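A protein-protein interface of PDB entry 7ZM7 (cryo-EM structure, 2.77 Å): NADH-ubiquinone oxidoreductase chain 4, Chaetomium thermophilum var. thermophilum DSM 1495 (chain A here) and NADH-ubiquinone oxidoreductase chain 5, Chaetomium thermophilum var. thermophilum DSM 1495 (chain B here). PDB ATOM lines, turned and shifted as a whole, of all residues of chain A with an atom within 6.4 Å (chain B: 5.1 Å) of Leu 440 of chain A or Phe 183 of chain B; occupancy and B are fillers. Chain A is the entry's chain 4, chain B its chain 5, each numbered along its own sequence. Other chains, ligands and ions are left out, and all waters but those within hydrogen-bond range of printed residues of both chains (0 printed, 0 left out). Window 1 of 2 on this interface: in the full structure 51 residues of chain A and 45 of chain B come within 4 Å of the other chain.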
ATOM      1  N   ILE A 353      24.182  20.823 -18.675  1.00  0.00           N
ATOM      2  CA  ILE A 353      23.330  20.073 -19.644  1.00  0.00           C
ATOM      3  C   ILE A 353      24.065  19.969 -20.986  1.00  0.00           C
ATOM      4  O   ILE A 353      24.096  18.861 -21.551  1.00  0.00           O
ATOM      5  CB  ILE A 353      21.931  20.711 -19.764  1.00  0.00           C
ATOM      6  CG1 ILE A 353      21.230  20.789 -18.407  1.00  0.00           C
ATOM      7  CG2 ILE A 353      21.080  19.971 -20.782  1.00  0.00           C
ATOM      8  CD1 ILE A 353      20.945  19.440 -17.795  1.00  0.00           C
ATOM      9  N   GLY A 357      25.701  16.789 -22.993  1.00  0.00           N
ATOM     10  CA  GLY A 357      25.391  16.542 -24.388  1.00  0.00           C
ATOM     11  C   GLY A 357      26.610  16.286 -25.259  1.00  0.00           C
ATOM     12  O   GLY A 357      26.587  15.396 -26.109  1.00  0.00           O
ATOM     13  N   GLY A 365      22.633  14.757 -29.251  1.00  0.00           N
ATOM     14  CA  GLY A 365      23.122  15.486 -28.103  1.00  0.00           C
ATOM     15  C   GLY A 365      24.243  16.430 -28.453  1.00  0.00           C
ATOM     16  O   GLY A 365      24.500  17.388 -27.723  1.00  0.00           O
ATOM     17  N   GLY A 435      17.380  23.034 -27.335  1.00  0.00           N
ATOM     18  CA  GLY A 435      18.742  22.675 -26.919  1.00  0.00           C
ATOM     19  C   GLY A 435      18.722  21.709 -25.765  1.00  0.00           C
ATOM     20  O   GLY A 435      19.566  20.819 -25.746  1.00  0.00           O
ATOM     21  N   GLU A 436      17.780  21.877 -24.845  1.00  0.00           N
ATOM     22  CA  GLU A 436      17.649  20.980 -23.672  1.00  0.00           C
ATOM     23  C   GLU A 436      17.054  19.655 -24.135  1.00  0.00           C
ATOM     24  O   GLU A 436      17.630  18.631 -23.781  1.00  0.00           O
ATOM     25  CB  GLU A 436      16.830  21.663 -22.581  1.00  0.00           C
ATOM     26  CG  GLU A 436      16.968  21.014 -21.219  1.00  0.00           C
ATOM     27  CD  GLU A 436      17.822  21.782 -20.229  1.00  0.00           C
ATOM     28  OE1 GLU A 436      18.468  22.761 -20.644  1.00  0.00           O
ATOM     29  OE2 GLU A 436      17.829  21.402 -19.046  1.00  0.00           O
ATOM     30  N   PHE A 437      16.104  19.613 -24.939  1.00  0.00           N
ATOM     31  CA  PHE A 437      15.490  18.367 -25.370  1.00  0.00           C
ATOM     32  C   PHE A 437      16.501  17.466 -26.055  1.00  0.00           C
ATOM     33  O   PHE A 437      16.565  16.263 -25.787  1.00  0.00           O
ATOM     34  CB  PHE A 437      14.320  18.668 -26.305  1.00  0.00           C
ATOM     35  CG  PHE A 437      13.460  17.484 -26.588  1.00  0.00           C
ATOM     36  CD1 PHE A 437      12.541  17.033 -25.658  1.00  0.00           C
ATOM     37  CD2 PHE A 437      13.582  16.809 -27.778  1.00  0.00           C
ATOM     38  CE1 PHE A 437      11.766  15.944 -25.921  1.00  0.00           C
ATOM     39  CE2 PHE A 437      12.817  15.721 -28.033  1.00  0.00           C
ATOM     40  CZ  PHE A 437      11.904  15.285 -27.106  1.00  0.00           C
ATOM     41  N   MET A 438      17.303  18.028 -26.946  1.00  0.00           N
ATOM     42  CA  MET A 438      18.284  17.225 -27.655  1.00  0.00           C
ATOM     43  C   MET A 438      19.494  16.913 -26.792  1.00  0.00           C
ATOM     44  O   MET A 438      20.076  15.838 -26.913  1.00  0.00           O
ATOM     45  CB  MET A 438      18.702  17.940 -28.928  1.00  0.00           C
ATOM     46  CG  MET A 438      17.834  17.651 -30.121  1.00  0.00           C
ATOM     47  SD  MET A 438      17.936  18.978 -31.331  1.00  0.00           S
ATOM     48  CE  MET A 438      19.302  18.414 -32.323  1.00  0.00           C
ATOM     49  N   SER A 439      19.885  17.831 -25.919  1.00  0.00           N
ATOM     50  CA  SER A 439      20.969  17.530 -24.996  1.00  0.00           C
ATOM     51  C   SER A 439      20.584  16.411 -24.045  1.00  0.00           C
ATOM     52  O   SER A 439      21.369  15.488 -23.813  1.00  0.00           O
ATOM     53  CB  SER A 439      21.347  18.772 -24.213  1.00  0.00           C
ATOM     54  OG  SER A 439      22.176  19.612 -24.967  1.00  0.00           O
ATOM     55  N   LEU A 440      19.380  16.475 -23.483  1.00  0.00           N
ATOM     56  CA  LEU A 440      18.971  15.461 -22.524  1.00  0.00           C
ATOM     57  C   LEU A 440      18.788  14.117 -23.196  1.00  0.00           C
ATOM     58  O   LEU A 440      19.131  13.081 -22.619  1.00  0.00           O
ATOM     59  CB  LEU A 440      17.693  15.893 -21.818  1.00  0.00           C
ATOM     60  CG  LEU A 440      17.818  17.085 -20.864  1.00  0.00           C
ATOM     61  CD1 LEU A 440      16.494  17.372 -20.223  1.00  0.00           C
ATOM     62  CD2 LEU A 440      18.878  16.889 -19.794  1.00  0.00           C
ATOM     63  N   TYR A 441      18.262  14.107 -24.419  1.00  0.00           N
ATOM     64  CA  TYR A 441      18.060  12.844 -25.114  1.00  0.00           C
ATOM     65  C   TYR A 441      19.374  12.092 -25.276  1.00  0.00           C
ATOM     66  O   TYR A 441      19.458  10.903 -24.962  1.00  0.00           O
ATOM     67  CB  TYR A 441      17.408  13.074 -26.476  1.00  0.00           C
ATOM     68  CG  TYR A 441      17.412  11.818 -27.300  1.00  0.00           C
ATOM     69  CD1 TYR A 441      16.438  10.857 -27.128  1.00  0.00           C
ATOM     70  CD2 TYR A 441      18.409  11.565 -28.213  1.00  0.00           C
ATOM     71  CE1 TYR A 441      16.452   9.711 -27.845  1.00  0.00           C
ATOM     72  CE2 TYR A 441      18.429  10.408 -28.917  1.00  0.00           C
ATOM     73  CZ  TYR A 441      17.449   9.482 -28.725  1.00  0.00           C
ATOM     74  OH  TYR A 441      17.453   8.324 -29.454  1.00  0.00           O
ATOM     75  N   GLY A 442      20.408  12.760 -25.782  1.00  0.00           N
ATOM     76  CA  GLY A 442      21.685  12.091 -25.954  1.00  0.00           C
ATOM     77  C   GLY A 442      22.311  11.678 -24.636  1.00  0.00           C
ATOM     78  O   GLY A 442      22.869  10.587 -24.519  1.00  0.00           O
ATOM     79  N   THR A 443      22.203  12.523 -23.617  1.00  0.00           N
ATOM     80  CA  THR A 443      22.700  12.115 -22.279  1.00  0.00           C
ATOM     81  C   THR A 443      22.037  10.786 -21.887  1.00  0.00           C
ATOM     82  O   THR A 443      22.756   9.889 -21.423  1.00  0.00           O
ATOM     83  CB  THR A 443      22.537  13.258 -21.266  1.00  0.00           C
ATOM     84  OG1 THR A 443      23.202  14.411 -21.781  1.00  0.00           O
ATOM     85  CG2 THR A 443      23.061  12.930 -19.888  1.00  0.00           C
ATOM     86  N   LEU A 444      20.720  10.668 -22.069  1.00  0.00           N
ATOM     87  CA  LEU A 444      19.972   9.430 -21.712  1.00  0.00           C
ATOM     88  C   LEU A 444      20.374   8.230 -22.574  1.00  0.00           C
ATOM     89  O   LEU A 444      20.583   7.156 -22.014  1.00  0.00           O
ATOM     90  CB  LEU A 444      18.474   9.713 -21.866  1.00  0.00           C
ATOM     91  CG  LEU A 444      17.549   8.583 -21.414  1.00  0.00           C
ATOM     92  CD1 LEU A 444      16.958   8.884 -20.047  1.00  0.00           C
ATOM     93  CD2 LEU A 444      16.448   8.344 -22.433  1.00  0.00           C
ATOM     94  N   GLU A 445      20.490   8.403 -23.888  1.00  0.00           N
ATOM     95  CA  GLU A 445      20.781   7.246 -24.777  1.00  0.00           C
ATOM     96  C   GLU A 445      22.168   6.690 -24.441  1.00  0.00           C
ATOM     97  O   GLU A 445      22.342   5.462 -24.510  1.00  0.00           O
ATOM     98  CB  GLU A 445      20.647   7.650 -26.246  1.00  0.00           C
ATOM     99  CG  GLU A 445      20.968   6.525 -27.212  1.00  0.00           C
ATOM    100  CD  GLU A 445      20.663   6.807 -28.671  1.00  0.00           C
ATOM    101  OE1 GLU A 445      20.643   7.992 -29.053  1.00  0.00           O
ATOM    102  OE2 GLU A 445      20.436   5.840 -29.421  1.00  0.00           O
ATOM    103  N   GLY A 451      21.093  10.948 -17.328  1.00  0.00           N
ATOM    104  CA  GLY A 451      20.113  11.749 -18.089  1.00  0.00           C
ATOM    105  C   GLY A 451      18.845  11.925 -17.273  1.00  0.00           C
ATOM    106  O   GLY A 451      18.248  13.015 -17.336  1.00  0.00           O
ATOM    107  N   ALA A 454      19.711  14.417 -14.820  1.00  0.00           N
ATOM    108  CA  ALA A 454      19.896  15.687 -15.557  1.00  0.00           C
ATOM    109  C   ALA A 454      18.524  16.265 -15.888  1.00  0.00           C
ATOM    110  O   ALA A 454      18.386  17.486 -15.845  1.00  0.00           O
ATOM    111  CB  ALA A 454      20.740  15.469 -16.790  1.00  0.00           C
ATOM    112  N   SER A 455      17.545  15.405 -16.171  1.00  0.00           N
ATOM    113  CA  SER A 455      16.178  15.851 -16.546  1.00  0.00           C
ATOM    114  C   SER A 455      15.470  16.485 -15.351  1.00  0.00           C
ATOM    115  O   SER A 455      14.414  17.087 -15.552  1.00  0.00           O
ATOM    116  CB  SER A 455      15.381  14.703 -17.087  1.00  0.00           C
ATOM    117  OG  SER A 455      14.991  13.828 -16.043  1.00  0.00           O
ATOM    118  N   THR A 456      16.035  16.357 -14.154  1.00  0.00           N
ATOM    119  CA  THR A 456      15.432  17.042 -12.983  1.00  0.00           C
ATOM    120  C   THR A 456      15.468  18.534 -13.299  1.00  0.00           C
ATOM    121  O   THR A 456      14.579  19.241 -12.824  1.00  0.00           O
ATOM    122  CB  THR A 456      16.114  16.654 -11.668  1.00  0.00           C
ATOM    123  OG1 THR A 456      17.457  17.133 -11.703  1.00  0.00           O
ATOM    124  CG2 THR A 456      16.070  15.167 -11.401  1.00  0.00           C
ATOM    125  N   SER A 457      16.504  18.989 -14.009  1.00  0.00           N
ATOM    126  CA  SER A 457      16.553  20.398 -14.471  1.00  0.00           C
ATOM    127  C   SER A 457      15.151  20.851 -14.888  1.00  0.00           C
ATOM    128  O   SER A 457      14.753  21.929 -14.452  1.00  0.00           O
ATOM    129  CB  SER A 457      17.535  20.564 -15.599  1.00  0.00           C
ATOM    130  OG  SER A 457      17.181  19.757 -16.709  1.00  0.00           O
ATOM    131  N   ILE A 458      14.432  20.058 -15.685  1.00  0.00           N
ATOM    132  CA  ILE A 458      13.121  20.494 -16.153  1.00  0.00           C
ATOM    133  C   ILE A 458      12.291  21.015 -14.987  1.00  0.00           C
ATOM    134  O   ILE A 458      11.607  22.036 -15.100  1.00  0.00           O
ATOM    135  CB  ILE A 458      12.410  19.344 -16.889  1.00  0.00           C
ATOM    136  CG1 ILE A 458      13.116  19.044 -18.205  1.00  0.00           C
ATOM    137  CG2 ILE A 458      10.968  19.680 -17.130  1.00  0.00           C
ATOM    138  CD1 ILE A 458      12.993  17.624 -18.635  1.00  0.00           C
ATOM    139  N   THR B 179       8.480  14.131 -20.587  1.00  0.00           N
ATOM    140  CA  THR B 179       9.645  14.276 -21.453  1.00  0.00           C
ATOM    141  C   THR B 179      10.529  13.035 -21.414  1.00  0.00           C
ATOM    142  O   THR B 179      11.080  12.630 -22.440  1.00  0.00           O
ATOM    143  CB  THR B 179      10.440  15.519 -21.059  1.00  0.00           C
ATOM    144  OG1 THR B 179       9.566  16.646 -20.980  1.00  0.00           O
ATOM    145  CG2 THR B 179      11.512  15.823 -22.077  1.00  0.00           C
ATOM    146  N   VAL B 180      10.690  12.433 -20.237  1.00  0.00           N
ATOM    147  CA  VAL B 180      11.447  11.188 -20.120  1.00  0.00           C
ATOM    148  C   VAL B 180      10.790  10.091 -20.935  1.00  0.00           C
ATOM    149  O   VAL B 180      11.465   9.321 -21.622  1.00  0.00           O
ATOM    150  CB  VAL B 180      11.573  10.779 -18.640  1.00  0.00           C
ATOM    151  CG1 VAL B 180      12.112   9.396 -18.518  1.00  0.00           C
ATOM    152  CG2 VAL B 180      12.463  11.751 -17.914  1.00  0.00           C
ATOM    153  N   GLY B 181       9.461   9.999 -20.867  1.00  0.00           N
ATOM    154  CA  GLY B 181       8.754   9.042 -21.694  1.00  0.00           C
ATOM    155  C   GLY B 181       8.866   9.333 -23.175  1.00  0.00           C
ATOM    156  O   GLY B 181       8.909   8.413 -23.991  1.00  0.00           O
ATOM    157  N   MET B 182       8.894  10.616 -23.546  1.00  0.00           N
ATOM    158  CA  MET B 182       9.113  10.980 -24.943  1.00  0.00           C
ATOM    159  C   MET B 182      10.516  10.621 -25.407  1.00  0.00           C
ATOM    160  O   MET B 182      10.721  10.362 -26.594  1.00  0.00           O
ATOM    161  CB  MET B 182       8.862  12.470 -25.161  1.00  0.00           C
ATOM    162  CG  MET B 182       7.425  12.849 -25.407  1.00  0.00           C
ATOM    163  SD  MET B 182       7.278  14.620 -25.658  1.00  0.00           S
ATOM    164  CE  MET B 182       7.008  15.171 -23.981  1.00  0.00           C
ATOM    165  N   PHE B 183      11.487  10.583 -24.491  1.00  0.00           N
ATOM    166  CA  PHE B 183      12.856  10.175 -24.899  1.00  0.00           C
ATOM    167  C   PHE B 183      12.898   8.662 -25.105  1.00  0.00           C
ATOM    168  O   PHE B 183      13.687   8.211 -25.951  1.00  0.00           O
ATOM    169  CB  PHE B 183      13.876  10.521 -23.811  1.00  0.00           C
ATOM    170  CG  PHE B 183      14.157  11.988 -23.628  1.00  0.00           C
ATOM    171  CD1 PHE B 183      14.099  12.862 -24.700  1.00  0.00           C
ATOM    172  CD2 PHE B 183      14.500  12.490 -22.384  1.00  0.00           C
ATOM    173  CE1 PHE B 183      14.367  14.209 -24.526  1.00  0.00           C
ATOM    174  CE2 PHE B 183      14.763  13.838 -22.212  1.00  0.00           C
ATOM    175  CZ  PHE B 183      14.697  14.695 -23.285  1.00  0.00           C
ATOM    176  N   ALA B 184      12.044   7.919 -24.402  1.00  0.00           N
ATOM    177  CA  ALA B 184      11.968   6.455 -24.606  1.00  0.00           C
ATOM    178  C   ALA B 184      11.465   6.146 -26.020  1.00  0.00           C
ATOM    179  O   ALA B 184      12.012   5.228 -26.644  1.00  0.00           O
ATOM    180  CB  ALA B 184      11.088   5.836 -23.552  1.00  0.00           C
ATOM    181  N   ILE B 185      10.457   6.888 -26.493  1.00  0.00           N
ATOM    182  CA  ILE B 185       9.867   6.638 -27.843  1.00  0.00           C
ATOM    183  C   ILE B 185      10.910   6.908 -28.931  1.00  0.00           C
ATOM    184  O   ILE B 185      11.020   6.082 -29.851  1.00  0.00           O
ATOM    185  CB  ILE B 185       8.606   7.501 -28.044  1.00  0.00           C
ATOM    186  CG1 ILE B 185       7.582   7.286 -26.927  1.00  0.00           C
ATOM    187  CG2 ILE B 185       7.996   7.264 -29.414  1.00  0.00           C
ATOM    188  CD1 ILE B 185       6.339   8.134 -27.063  1.00  0.00           C
ATOM    189  N   LEU B 186      11.650   8.014 -28.821  1.00  0.00           N
ATOM    190  CA  LEU B 186      12.700   8.354 -29.817  1.00  0.00           C
ATOM    191  C   LEU B 186      13.807   7.302 -29.770  1.00  0.00           C
ATOM    192  O   LEU B 186      14.288   6.904 -30.838  1.00  0.00           O
ATOM    193  CB  LEU B 186      13.259   9.741 -29.496  1.00  0.00           C
ATOM    194  CG  LEU B 186      12.374  10.919 -29.890  1.00  0.00           C
ATOM    195  CD1 LEU B 186      12.948  12.220 -29.356  1.00  0.00           C
ATOM    196  CD2 LEU B 186      12.204  10.986 -31.399  1.00  0.00           C
ATOM    197  N   TRP B 187      14.198   6.880 -28.565  1.00  0.00           N
ATOM    198  CA  TRP B 187      15.255   5.848 -28.406  1.00  0.00           C
ATOM    199  C   TRP B 187      14.781   4.516 -28.990  1.00  0.00           C
ATOM    200  O   TRP B 187      15.590   3.844 -29.635  1.00  0.00           O
ATOM    201  CB  TRP B 187      15.652   5.724 -26.933  1.00  0.00           C
ATOM    202  CG  TRP B 187      16.916   4.956 -26.699  1.00  0.00           C
ATOM    203  CD1 TRP B 187      17.763   4.452 -27.642  1.00  0.00           C
ATOM    204  CD2 TRP B 187      17.483   4.606 -25.426  1.00  0.00           C
ATOM    205  NE1 TRP B 187      18.809   3.806 -27.046  1.00  0.00           N
ATOM    206  CE2 TRP B 187      18.667   3.885 -25.688  1.00  0.00           C
ATOM    207  CE3 TRP B 187      17.109   4.829 -24.098  1.00  0.00           C
ATOM    208  CZ2 TRP B 187      19.477   3.389 -24.668  1.00  0.00           C
ATOM    209  CZ3 TRP B 187      17.908   4.336 -23.093  1.00  0.00           C
ATOM    210  CH2 TRP B 187      19.073   3.626 -23.377  1.00  0.00           C
ATOM    211  N   SER B 188      13.506   4.174 -28.811  1.00  0.00           N
ATOM    212  CA  SER B 188      12.995   2.846 -29.241  1.00  0.00           C
ATOM    213  C   SER B 188      12.594   2.831 -30.711  1.00  0.00           C
ATOM    214  O   SER B 188      12.915   1.836 -31.386  1.00  0.00           O
ATOM    215  CB  SER B 188      11.844   2.401 -28.378  1.00  0.00           C
ATOM    216  OG  SER B 188      10.712   3.233 -28.576  1.00  0.00           O
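The side-chain hydroxyl (OH) of Tyr 441 of chain A is in hydrogen-bond range of the side-chain carboxylate (OE1) of Glu 445 of chain A (3.2 Å).
Printed residues of chain B that touch a printed residue of chain A: Thr 179, Val 180, Phe 183, Leu 186 and Trp 187. Hydrophobic or aromatic side chains of chain B within 4 Å of the printed part of chain A: Val 180, Phe 183, Leu 186 and Trp 187. Along chain B the printed residues that touch a printed residue of chain A span positions 179 to 187. Printed residues of chain A that touch a printed residue of chain B: Phe 437, Leu 440, Tyr 441, Leu 444, Glu 445 and Ser 455. Hydrophobic or aromatic side chains of chain A within 4 Å of the printed part of chain B: Phe 437, Leu 440, Tyr 441 and Leu 444. Along chain A the printed residues that touch a printed residue of chain B span positions 437 to 455. Among the printed residues, 11 pairs touch across the chains.
Among the printed residues, merely in contact across the chains: Phe 437 of chain A with Thr 179 of chain B (3.9 Å), Phe 437 of chain A with Phe 183 of chain B (3.3 Å), Phe 437 of chain A with Leu 186 of chain B (3.7 Å), Leu 440 of chain A with Phe 183 of chain B (3.5 Å), Tyr 441 of chain A with Phe 183 of chain B (3.7 Å), Tyr 441 of chain A with Leu 186 of chain B (3.6 Å), Tyr 441 of chain A with Trp 187 of chain B (3.5 Å), Leu 444 of chain A with Phe 183 of chain B (3.6 Å), Leu 444 of chain A with Trp 187 of chain B (3.9 Å), Glu 445 of chain A with Trp 187 of chain B (3.5 Å) and Ser 455 of chain A with Val 180 of chain B (3.8 Å).
Leu 440 of chain A touches just one residue of chain B: Phe 183 (3.5 Å). Phe 183 of chain B touches just these residues of chain A: Phe 437, Leu 440, Tyr 441 and Leu 444. Of the printed residues of chain B, Phe 437 of chain A touches Thr 179, Phe 183 and Leu 186. Of the printed residues of chain B, Leu 444 of chain A touches Phe 183 and Trp 187. Printed residues of chain B within 4 Å of Ser 455 of chain A: Val 180. Of the printed residues of chain A, Thr 179 of chain B touches Phe 437 (3.9 Å). Of the printed residues of chain B, Glu 445 of chain A touches Trp 187. Ile 458 of chain A touches none of the printed residues of chain B. Glu 436 of chain A touches none of the printed residues of chain B. The nearest printed residue of chain B that does not touch Leu 440 of chain A is Thr 179 of chain B (5.5 Å).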
